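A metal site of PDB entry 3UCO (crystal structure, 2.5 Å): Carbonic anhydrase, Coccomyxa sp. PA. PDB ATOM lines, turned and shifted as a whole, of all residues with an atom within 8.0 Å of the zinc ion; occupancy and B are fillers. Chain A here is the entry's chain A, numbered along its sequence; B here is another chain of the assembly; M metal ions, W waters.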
ATOM      1  N   GLY A  46     -20.702 -14.506  -6.641  1.00  0.00           N
ATOM      2  CA  GLY A  46     -21.568 -13.931  -5.637  1.00  0.00           C
ATOM      3  C   GLY A  46     -22.276 -12.688  -6.142  1.00  0.00           C
ATOM      4  O   GLY A  46     -22.269 -12.390  -7.359  1.00  0.00           O
ATOM      5  N   CYS A  47     -22.808 -11.892  -5.218  1.00  0.00           N
ATOM      6  CA  CYS A  47     -23.706 -10.820  -5.544  1.00  0.00           C
ATOM      7  C   CYS A  47     -23.004  -9.561  -5.802  1.00  0.00           C
ATOM      8  O   CYS A  47     -21.953  -9.314  -5.215  1.00  0.00           O
ATOM      9  CB  CYS A  47     -24.803 -10.669  -4.474  1.00  0.00           C
ATOM     10  SG  CYS A  47     -26.118  -9.558  -5.035  1.00  0.00           S
ATOM     11  N   ALA A  48     -23.535  -8.773  -6.746  1.00  0.00           N
ATOM     12  CA  ALA A  48     -22.977  -7.436  -7.061  1.00  0.00           C
ATOM     13  C   ALA A  48     -23.077  -6.461  -5.876  1.00  0.00           C
ATOM     14  O   ALA A  48     -22.429  -5.408  -5.910  1.00  0.00           O
ATOM     15  CB  ALA A  48     -23.623  -6.865  -8.245  1.00  0.00           C
ATOM     16  N   ASP A  49     -23.846  -6.803  -4.862  1.00  0.00           N
ATOM     17  CA  ASP A  49     -24.059  -6.019  -3.660  1.00  0.00           C
ATOM     18  C   ASP A  49     -22.805  -5.360  -3.107  1.00  0.00           C
ATOM     19  O   ASP A  49     -21.800  -6.005  -2.976  1.00  0.00           O
ATOM     20  CB  ASP A  49     -24.652  -6.933  -2.602  1.00  0.00           C
ATOM     21  CG  ASP A  49     -25.244  -6.196  -1.458  1.00  0.00           C
ATOM     22  OD1 ASP A  49     -24.495  -5.699  -0.649  1.00  0.00           O
ATOM     23  OD2 ASP A  49     -26.459  -6.120  -1.361  1.00  0.00           O
ATOM     24  N   SER A  50     -22.886  -4.083  -2.748  1.00  0.00           N
ATOM     25  CA  SER A  50     -21.703  -3.342  -2.286  1.00  0.00           C
ATOM     26  C   SER A  50     -21.173  -3.684  -0.870  1.00  0.00           C
ATOM     27  O   SER A  50     -20.110  -3.160  -0.451  1.00  0.00           O
ATOM     28  CB  SER A  50     -21.988  -1.855  -2.367  1.00  0.00           C
ATOM     29  OG  SER A  50     -22.974  -1.545  -1.428  1.00  0.00           O
ATOM     30  N   ARG A  51     -21.867  -4.553  -0.144  1.00  0.00           N
ATOM     31  CA  ARG A  51     -21.373  -4.967   1.165  1.00  0.00           C
ATOM     32  C   ARG A  51     -20.703  -6.315   1.108  1.00  0.00           C
ATOM     33  O   ARG A  51     -20.410  -6.857   2.147  1.00  0.00           O
ATOM     34  CB  ARG A  51     -22.526  -5.001   2.200  1.00  0.00           C
ATOM     35  CG  ARG A  51     -23.327  -3.684   2.224  1.00  0.00           C
ATOM     36  CD  ARG A  51     -24.719  -3.846   2.727  1.00  0.00           C
ATOM     37  NE  ARG A  51     -25.522  -4.823   1.994  1.00  0.00           N
ATOM     38  CZ  ARG A  51     -26.818  -5.035   2.240  1.00  0.00           C
ATOM     39  NH1 ARG A  51     -27.436  -4.352   3.212  1.00  0.00           N
ATOM     40  NH2 ARG A  51     -27.506  -5.929   1.545  1.00  0.00           N
ATOM     41  N   VAL A  52     -20.457  -6.871  -0.078  1.00  0.00           N
ATOM     42  CA  VAL A  52     -19.951  -8.254  -0.120  1.00  0.00           C
ATOM     43  C   VAL A  52     -18.711  -8.430  -1.029  1.00  0.00           C
ATOM     44  O   VAL A  52     -18.893  -8.844  -2.198  1.00  0.00           O
ATOM     45  CB  VAL A  52     -21.085  -9.271  -0.497  1.00  0.00           C
ATOM     46  CG1 VAL A  52     -20.710 -10.714  -0.134  1.00  0.00           C
ATOM     47  CG2 VAL A  52     -22.391  -8.916   0.170  1.00  0.00           C
ATOM     48  N   ASN A  70     -22.853 -10.672  -9.974  1.00  0.00           N
ATOM     49  CA  ASN A  70     -24.009 -10.262 -10.669  1.00  0.00           C
ATOM     50  C   ASN A  70     -25.166 -10.042  -9.679  1.00  0.00           C
ATOM     51  O   ASN A  70     -25.026 -10.295  -8.429  1.00  0.00           O
ATOM     52  CB  ASN A  70     -24.306 -11.288 -11.765  1.00  0.00           C
ATOM     53  CG  ASN A  70     -24.795 -12.573 -11.250  1.00  0.00           C
ATOM     54  OD1 ASN A  70     -25.672 -12.604 -10.407  1.00  0.00           O
ATOM     55  ND2 ASN A  70     -24.316 -13.680 -11.780  1.00  0.00           N
ATOM     56  N   VAL A  71     -26.288  -9.554 -10.164  1.00  0.00           N
ATOM     57  CA  VAL A  71     -27.392  -9.246  -9.292  1.00  0.00           C
ATOM     58  C   VAL A  71     -28.047 -10.553  -8.840  1.00  0.00           C
ATOM     59  O   VAL A  71     -28.769 -11.143  -9.581  1.00  0.00           O
ATOM     60  CB  VAL A  71     -28.432  -8.236  -9.924  1.00  0.00           C
ATOM     61  CG1 VAL A  71     -29.731  -8.165  -9.101  1.00  0.00           C
ATOM     62  CG2 VAL A  71     -27.836  -6.873 -10.038  1.00  0.00           C
ATOM     63  N   GLY A  72     -27.843 -10.963  -7.582  1.00  0.00           N
ATOM     64  CA  GLY A  72     -28.514 -12.137  -7.025  1.00  0.00           C
ATOM     65  C   GLY A  72     -27.692 -13.405  -7.183  1.00  0.00           C
ATOM     66  O   GLY A  72     -28.225 -14.498  -7.051  1.00  0.00           O
ATOM     67  N   ASN A  73     -26.382 -13.260  -7.449  1.00  0.00           N
ATOM     68  CA  ASN A  73     -25.504 -14.422  -7.592  1.00  0.00           C
ATOM     69  C   ASN A  73     -26.115 -15.619  -8.378  1.00  0.00           C
ATOM     70  O   ASN A  73     -26.123 -16.780  -7.875  1.00  0.00           O
ATOM     71  CB  ASN A  73     -24.955 -14.900  -6.230  1.00  0.00           C
ATOM     72  CG  ASN A  73     -26.030 -15.043  -5.183  1.00  0.00           C
ATOM     73  OD1 ASN A  73     -26.315 -14.085  -4.470  1.00  0.00           O
ATOM     74  ND2 ASN A  73     -26.605 -16.257  -5.041  1.00  0.00           N
ATOM     75  N   CYS A 101     -21.761 -17.965  -3.467  1.00  0.00           N
ATOM     76  CA  CYS A 101     -22.052 -17.227  -2.259  1.00  0.00           C
ATOM     77  C   CYS A 101     -23.274 -16.321  -2.412  1.00  0.00           C
ATOM     78  O   CYS A 101     -23.267 -15.440  -3.236  1.00  0.00           O
ATOM     79  CB  CYS A 101     -20.835 -16.375  -1.887  1.00  0.00           C
ATOM     80  SG  CYS A 101     -20.996 -15.312  -0.415  1.00  0.00           S
ATOM     81  N   GLY A 102     -24.278 -16.527  -1.554  1.00  0.00           N
ATOM     82  CA  GLY A 102     -25.421 -15.611  -1.471  1.00  0.00           C
ATOM     83  C   GLY A 102     -25.283 -14.854  -0.159  1.00  0.00           C
ATOM     84  O   GLY A 102     -24.299 -15.070   0.575  1.00  0.00           O
ATOM     85  N   HIS A 103     -26.254 -13.980   0.128  1.00  0.00           N
ATOM     86  CA  HIS A 103     -26.167 -13.152   1.315  1.00  0.00           C
ATOM     87  C   HIS A 103     -27.546 -12.619   1.877  1.00  0.00           C
ATOM     88  O   HIS A 103     -28.464 -12.282   1.108  1.00  0.00           O
ATOM     89  CB  HIS A 103     -25.220 -11.988   1.007  1.00  0.00           C
ATOM     90  CG  HIS A 103     -25.847 -10.923   0.161  1.00  0.00           C
ATOM     91  ND1 HIS A 103     -26.461  -9.808   0.708  1.00  0.00           N
ATOM     92  CD2 HIS A 103     -25.984 -10.817  -1.179  1.00  0.00           C
ATOM     93  CE1 HIS A 103     -26.905  -9.033  -0.267  1.00  0.00           C
ATOM     94  NE2 HIS A 103     -26.634  -9.617  -1.418  1.00  0.00           N
ATOM     95  N   TYR A 104     -27.687 -12.531   3.194  1.00  0.00           N
ATOM     96  CA  TYR A 104     -28.932 -12.035   3.742  1.00  0.00           C
ATOM     97  C   TYR A 104     -29.115 -10.576   3.349  1.00  0.00           C
ATOM     98  O   TYR A 104     -28.147  -9.874   3.079  1.00  0.00           O
ATOM     99  CB  TYR A 104     -28.942 -12.207   5.249  1.00  0.00           C
ATOM    100  CG  TYR A 104     -28.904 -13.652   5.546  1.00  0.00           C
ATOM    101  CD1 TYR A 104     -27.780 -14.264   6.141  1.00  0.00           C
ATOM    102  CD2 TYR A 104     -29.972 -14.451   5.156  1.00  0.00           C
ATOM    103  CE1 TYR A 104     -27.756 -15.649   6.355  1.00  0.00           C
ATOM    104  CE2 TYR A 104     -29.969 -15.796   5.367  1.00  0.00           C
ATOM    105  CZ  TYR A 104     -28.872 -16.390   5.954  1.00  0.00           C
ATOM    106  OH  TYR A 104     -28.970 -17.708   6.114  1.00  0.00           O
ATOM    107  N   ASN A 105     -30.360 -10.124   3.272  1.00  0.00           N
ATOM    108  CA  ASN A 105     -30.643  -8.746   2.905  1.00  0.00           C
ATOM    109  C   ASN A 105     -30.364  -8.477   1.404  1.00  0.00           C
ATOM    110  O   ASN A 105     -30.089  -7.337   0.975  1.00  0.00           O
ATOM    111  CB  ASN A 105     -29.939  -7.748   3.861  1.00  0.00           C
ATOM    112  CG  ASN A 105     -30.611  -6.385   3.863  1.00  0.00           C
ATOM    113  OD1 ASN A 105     -30.016  -5.366   3.425  1.00  0.00           O
ATOM    114  ND2 ASN A 105     -31.888  -6.342   4.306  1.00  0.00           N
ATOM    115  N   CYS A 106     -30.405  -9.546   0.613  1.00  0.00           N
ATOM    116  CA  CYS A 106     -30.142  -9.413  -0.827  1.00  0.00           C
ATOM    117  C   CYS A 106     -31.365  -8.829  -1.562  1.00  0.00           C
ATOM    118  O   CYS A 106     -32.444  -9.424  -1.575  1.00  0.00           O
ATOM    119  CB  CYS A 106     -29.739 -10.788  -1.359  1.00  0.00           C
ATOM    120  SG  CYS A 106     -29.556 -10.779  -3.191  1.00  0.00           S
ATOM    121  N   GLY A 107     -31.197  -7.679  -2.189  1.00  0.00           N
ATOM    122  CA  GLY A 107     -32.308  -6.996  -2.920  1.00  0.00           C
ATOM    123  C   GLY A 107     -32.909  -7.796  -4.065  1.00  0.00           C
ATOM    124  O   GLY A 107     -34.094  -7.711  -4.350  1.00  0.00           O
ATOM    125  N   ALA A 108     -32.099  -8.617  -4.686  1.00  0.00           N
ATOM    126  CA  ALA A 108     -32.556  -9.401  -5.773  1.00  0.00           C
ATOM    127  C   ALA A 108     -33.476 -10.494  -5.255  1.00  0.00           C
ATOM    128  O   ALA A 108     -34.439 -10.834  -5.893  1.00  0.00           O
ATOM    129  CB  ALA A 108     -31.346 -10.005  -6.529  1.00  0.00           C
ATOM    130  N   CYS A 109     -33.184 -11.078  -4.114  1.00  0.00           N
ATOM    131  CA  CYS A 109     -34.079 -12.093  -3.602  1.00  0.00           C
ATOM    132  C   CYS A 109     -35.367 -11.513  -3.040  1.00  0.00           C
ATOM    133  O   CYS A 109     -36.387 -12.152  -3.150  1.00  0.00           O
ATOM    134  CB  CYS A 109     -33.399 -12.964  -2.573  1.00  0.00           C
ATOM    135  SG  CYS A 109     -32.056 -13.897  -3.245  1.00  0.00           S
ATOM    136  N   LYS A 110     -35.314 -10.310  -2.476  1.00  0.00           N
ATOM    137  CA  LYS A 110     -36.556  -9.563  -2.157  1.00  0.00           C
ATOM    138  C   LYS A 110     -37.420  -9.281  -3.409  1.00  0.00           C
ATOM    139  O   LYS A 110     -38.591  -9.592  -3.433  1.00  0.00           O
ATOM    140  CB  LYS A 110     -36.206  -8.241  -1.436  1.00  0.00           C
ATOM    141  CG  LYS A 110     -37.258  -7.706  -0.399  1.00  0.00           C
ATOM    142  CD  LYS A 110     -38.076  -6.453  -0.833  1.00  0.00           C
ATOM    143  CE  LYS A 110     -37.514  -5.605  -2.093  1.00  0.00           C
ATOM    144  NZ  LYS A 110     -38.517  -4.694  -2.885  1.00  0.00           N
ATOM    145  N   TRP A 150     -37.825 -13.773   3.089  1.00  0.00           N
ATOM    146  CA  TRP A 150     -36.665 -13.177   2.507  1.00  0.00           C
ATOM    147  C   TRP A 150     -35.397 -14.022   2.836  1.00  0.00           C
ATOM    148  O   TRP A 150     -34.667 -14.413   1.913  1.00  0.00           O
ATOM    149  CB  TRP A 150     -36.534 -11.758   3.005  1.00  0.00           C
ATOM    150  CG  TRP A 150     -35.582 -10.966   2.236  1.00  0.00           C
ATOM    151  CD1 TRP A 150     -34.752 -11.404   1.209  1.00  0.00           C
ATOM    152  CD2 TRP A 150     -35.260  -9.587   2.448  1.00  0.00           C
ATOM    153  NE1 TRP A 150     -33.973 -10.373   0.764  1.00  0.00           N
ATOM    154  CE2 TRP A 150     -34.246  -9.240   1.488  1.00  0.00           C
ATOM    155  CE3 TRP A 150     -35.688  -8.619   3.361  1.00  0.00           C
ATOM    156  CZ2 TRP A 150     -33.695  -7.947   1.392  1.00  0.00           C
ATOM    157  CZ3 TRP A 150     -35.157  -7.303   3.258  1.00  0.00           C
ATOM    158  CH2 TRP A 150     -34.165  -6.994   2.274  1.00  0.00           C
ATOM    159  N   VAL A 154     -33.039 -16.541   0.164  1.00  0.00           N
ATOM    160  CA  VAL A 154     -31.606 -16.429   0.031  1.00  0.00           C
ATOM    161  C   VAL A 154     -30.951 -17.804  -0.006  1.00  0.00           C
ATOM    162  O   VAL A 154     -30.109 -18.124  -0.864  1.00  0.00           O
ATOM    163  CB  VAL A 154     -31.023 -15.560   1.147  1.00  0.00           C
ATOM    164  CG1 VAL A 154     -29.521 -15.786   1.267  1.00  0.00           C
ATOM    165  CG2 VAL A 154     -31.368 -14.069   0.924  1.00  0.00           C
ATOM    166  N   ASN A 157     -32.025 -19.940  -3.031  1.00  0.00           N
ATOM    167  CA  ASN A 157     -31.322 -19.509  -4.207  1.00  0.00           C
ATOM    168  C   ASN A 157     -29.886 -20.071  -4.240  1.00  0.00           C
ATOM    169  O   ASN A 157     -29.436 -20.568  -5.262  1.00  0.00           O
ATOM    170  CB  ASN A 157     -31.273 -18.017  -4.272  1.00  0.00           C
ATOM    171  CG  ASN A 157     -30.778 -17.530  -5.600  1.00  0.00           C
ATOM    172  OD1 ASN A 157     -31.167 -18.064  -6.623  1.00  0.00           O
ATOM    173  ND2 ASN A 157     -29.891 -16.515  -5.610  1.00  0.00           N
ATOM    174  N   PRO A 190     -24.283  -9.524   5.866  1.00  0.00           N
ATOM    175  CA  PRO A 190     -23.656  -8.177   5.889  1.00  0.00           C
ATOM    176  C   PRO A 190     -23.586  -7.521   7.320  1.00  0.00           C
ATOM    177  O   PRO A 190     -22.687  -6.712   7.595  1.00  0.00           O
ATOM    178  CB  PRO A 190     -24.533  -7.364   4.922  1.00  0.00           C
ATOM    179  CG  PRO A 190     -25.423  -8.392   4.218  1.00  0.00           C
ATOM    180  CD  PRO A 190     -25.509  -9.601   5.046  1.00  0.00           C
ATOM    181  N   GLN B  38     -27.933  -0.456   1.749  1.00  0.00           N
ATOM    182  CA  GLN B  38     -26.697   0.000   1.124  1.00  0.00           C
ATOM    183  C   GLN B  38     -26.964   1.327   0.411  1.00  0.00           C
ATOM    184  O   GLN B  38     -28.086   1.578  -0.097  1.00  0.00           O
ATOM    185  CB  GLN B  38     -26.139  -1.067   0.143  1.00  0.00           C
ATOM    186  CG  GLN B  38     -27.084  -1.388  -1.003  1.00  0.00           C
ATOM    187  CD  GLN B  38     -26.614  -2.502  -1.911  1.00  0.00           C
ATOM    188  OE1 GLN B  38     -25.405  -2.628  -2.233  1.00  0.00           O
ATOM    189  NE2 GLN B  38     -27.572  -3.309  -2.350  1.00  0.00           N
ATOM    190  N   PHE B  66     -20.680  -0.830  -5.461  1.00  0.00           N
ATOM    191  CA  PHE B  66     -21.494  -1.916  -6.108  1.00  0.00           C
ATOM    192  C   PHE B  66     -20.715  -2.427  -7.342  1.00  0.00           C
ATOM    193  O   PHE B  66     -20.213  -1.628  -8.199  1.00  0.00           O
ATOM    194  CB  PHE B  66     -22.879  -1.371  -6.473  1.00  0.00           C
ATOM    195  CG  PHE B  66     -23.942  -2.422  -6.759  1.00  0.00           C
ATOM    196  CD1 PHE B  66     -24.942  -2.707  -5.812  1.00  0.00           C
ATOM    197  CD2 PHE B  66     -24.033  -3.045  -8.014  1.00  0.00           C
ATOM    198  CE1 PHE B  66     -25.987  -3.608  -6.084  1.00  0.00           C
ATOM    199  CE2 PHE B  66     -25.076  -3.962  -8.288  1.00  0.00           C
ATOM    200  CZ  PHE B  66     -26.051  -4.230  -7.329  1.00  0.00           C
ATOM    201  N   TYR B  88     -30.209  -1.278 -11.987  1.00  0.00           N
ATOM    202  CA  TYR B  88     -30.521  -1.292 -10.577  1.00  0.00           C
ATOM    203  C   TYR B  88     -29.757  -0.249  -9.798  1.00  0.00           C
ATOM    204  O   TYR B  88     -30.281   0.289  -8.800  1.00  0.00           O
ATOM    205  CB  TYR B  88     -30.220  -2.634  -9.974  1.00  0.00           C
ATOM    206  CG  TYR B  88     -30.673  -2.805  -8.515  1.00  0.00           C
ATOM    207  CD1 TYR B  88     -32.052  -2.896  -8.184  1.00  0.00           C
ATOM    208  CD2 TYR B  88     -29.746  -2.922  -7.487  1.00  0.00           C
ATOM    209  CE1 TYR B  88     -32.482  -3.085  -6.884  1.00  0.00           C
ATOM    210  CE2 TYR B  88     -30.151  -3.127  -6.194  1.00  0.00           C
ATOM    211  CZ  TYR B  88     -31.512  -3.209  -5.872  1.00  0.00           C
ATOM    212  OH  TYR B  88     -31.889  -3.399  -4.552  1.00  0.00           O
HETATM  213 ZN    ZN M   1     -27.620  -9.418  -3.251  1.00  0.00          ZN
HETATM  214  O   HOH W   1     -28.170  -7.225  -3.499  1.00  0.00           O
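Merely in contact with the zinc ion: Asp 49. Within 4 Å of the zinc ion: Cys 47, Asp 49, His 103 and Cys 106. The nearest printed residue that does not touch the zinc ion is Gly 107 (4.1 Å).
The zinc ion is bound by a ring nitrogen (NE2) of His 103 (2.1 Å), water W1 (2.3 Å), the side-chain sulfur of Cys 47 (2.3 Å) and the side-chain sulfur of Cys 106 (2.4 Å). The zinc ion has four donor atoms within binding distance.
Water W1 lies within hydrogen-bond range of OD2 of Asp 49 (3.0 Å) and N of Gly 107 (3.3 Å).
The backbone NH (N) of Asp 49 sits close to the side-chain sulfur (SG) of Cys 47, at 3.6 Å. N of Gly 72 lies close to SG of Cys 47. O of Asn 70 sits close to SG of Cys 47, at 3.6 Å. The backbone NH (N) of Ala 108 lies close to the side-chain sulfur (SG) of Cys 106 (3.7 Å). The side-chain sulfur (SG) of Cys 106 sits close to the backbone NH (N) of Cys 109 (3.8 Å). The backbone carbonyl oxygen (O) of Cys 106 sits at hydrogen-bond distance from the indole nitrogen (NE1) of Trp 150 (3.0 Å). The side-chain carboxylate (OD1) of Asp 49 lies within salt-bridge range of the guanidinium group (NE) of Arg 51, at 3.0 Å. The side-chain amide nitrogen (NE2) of Gln 38 of chain B is in hydrogen-bond range of the side-chain carboxylate (OD2) of Asp 49 (3.2 Å).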
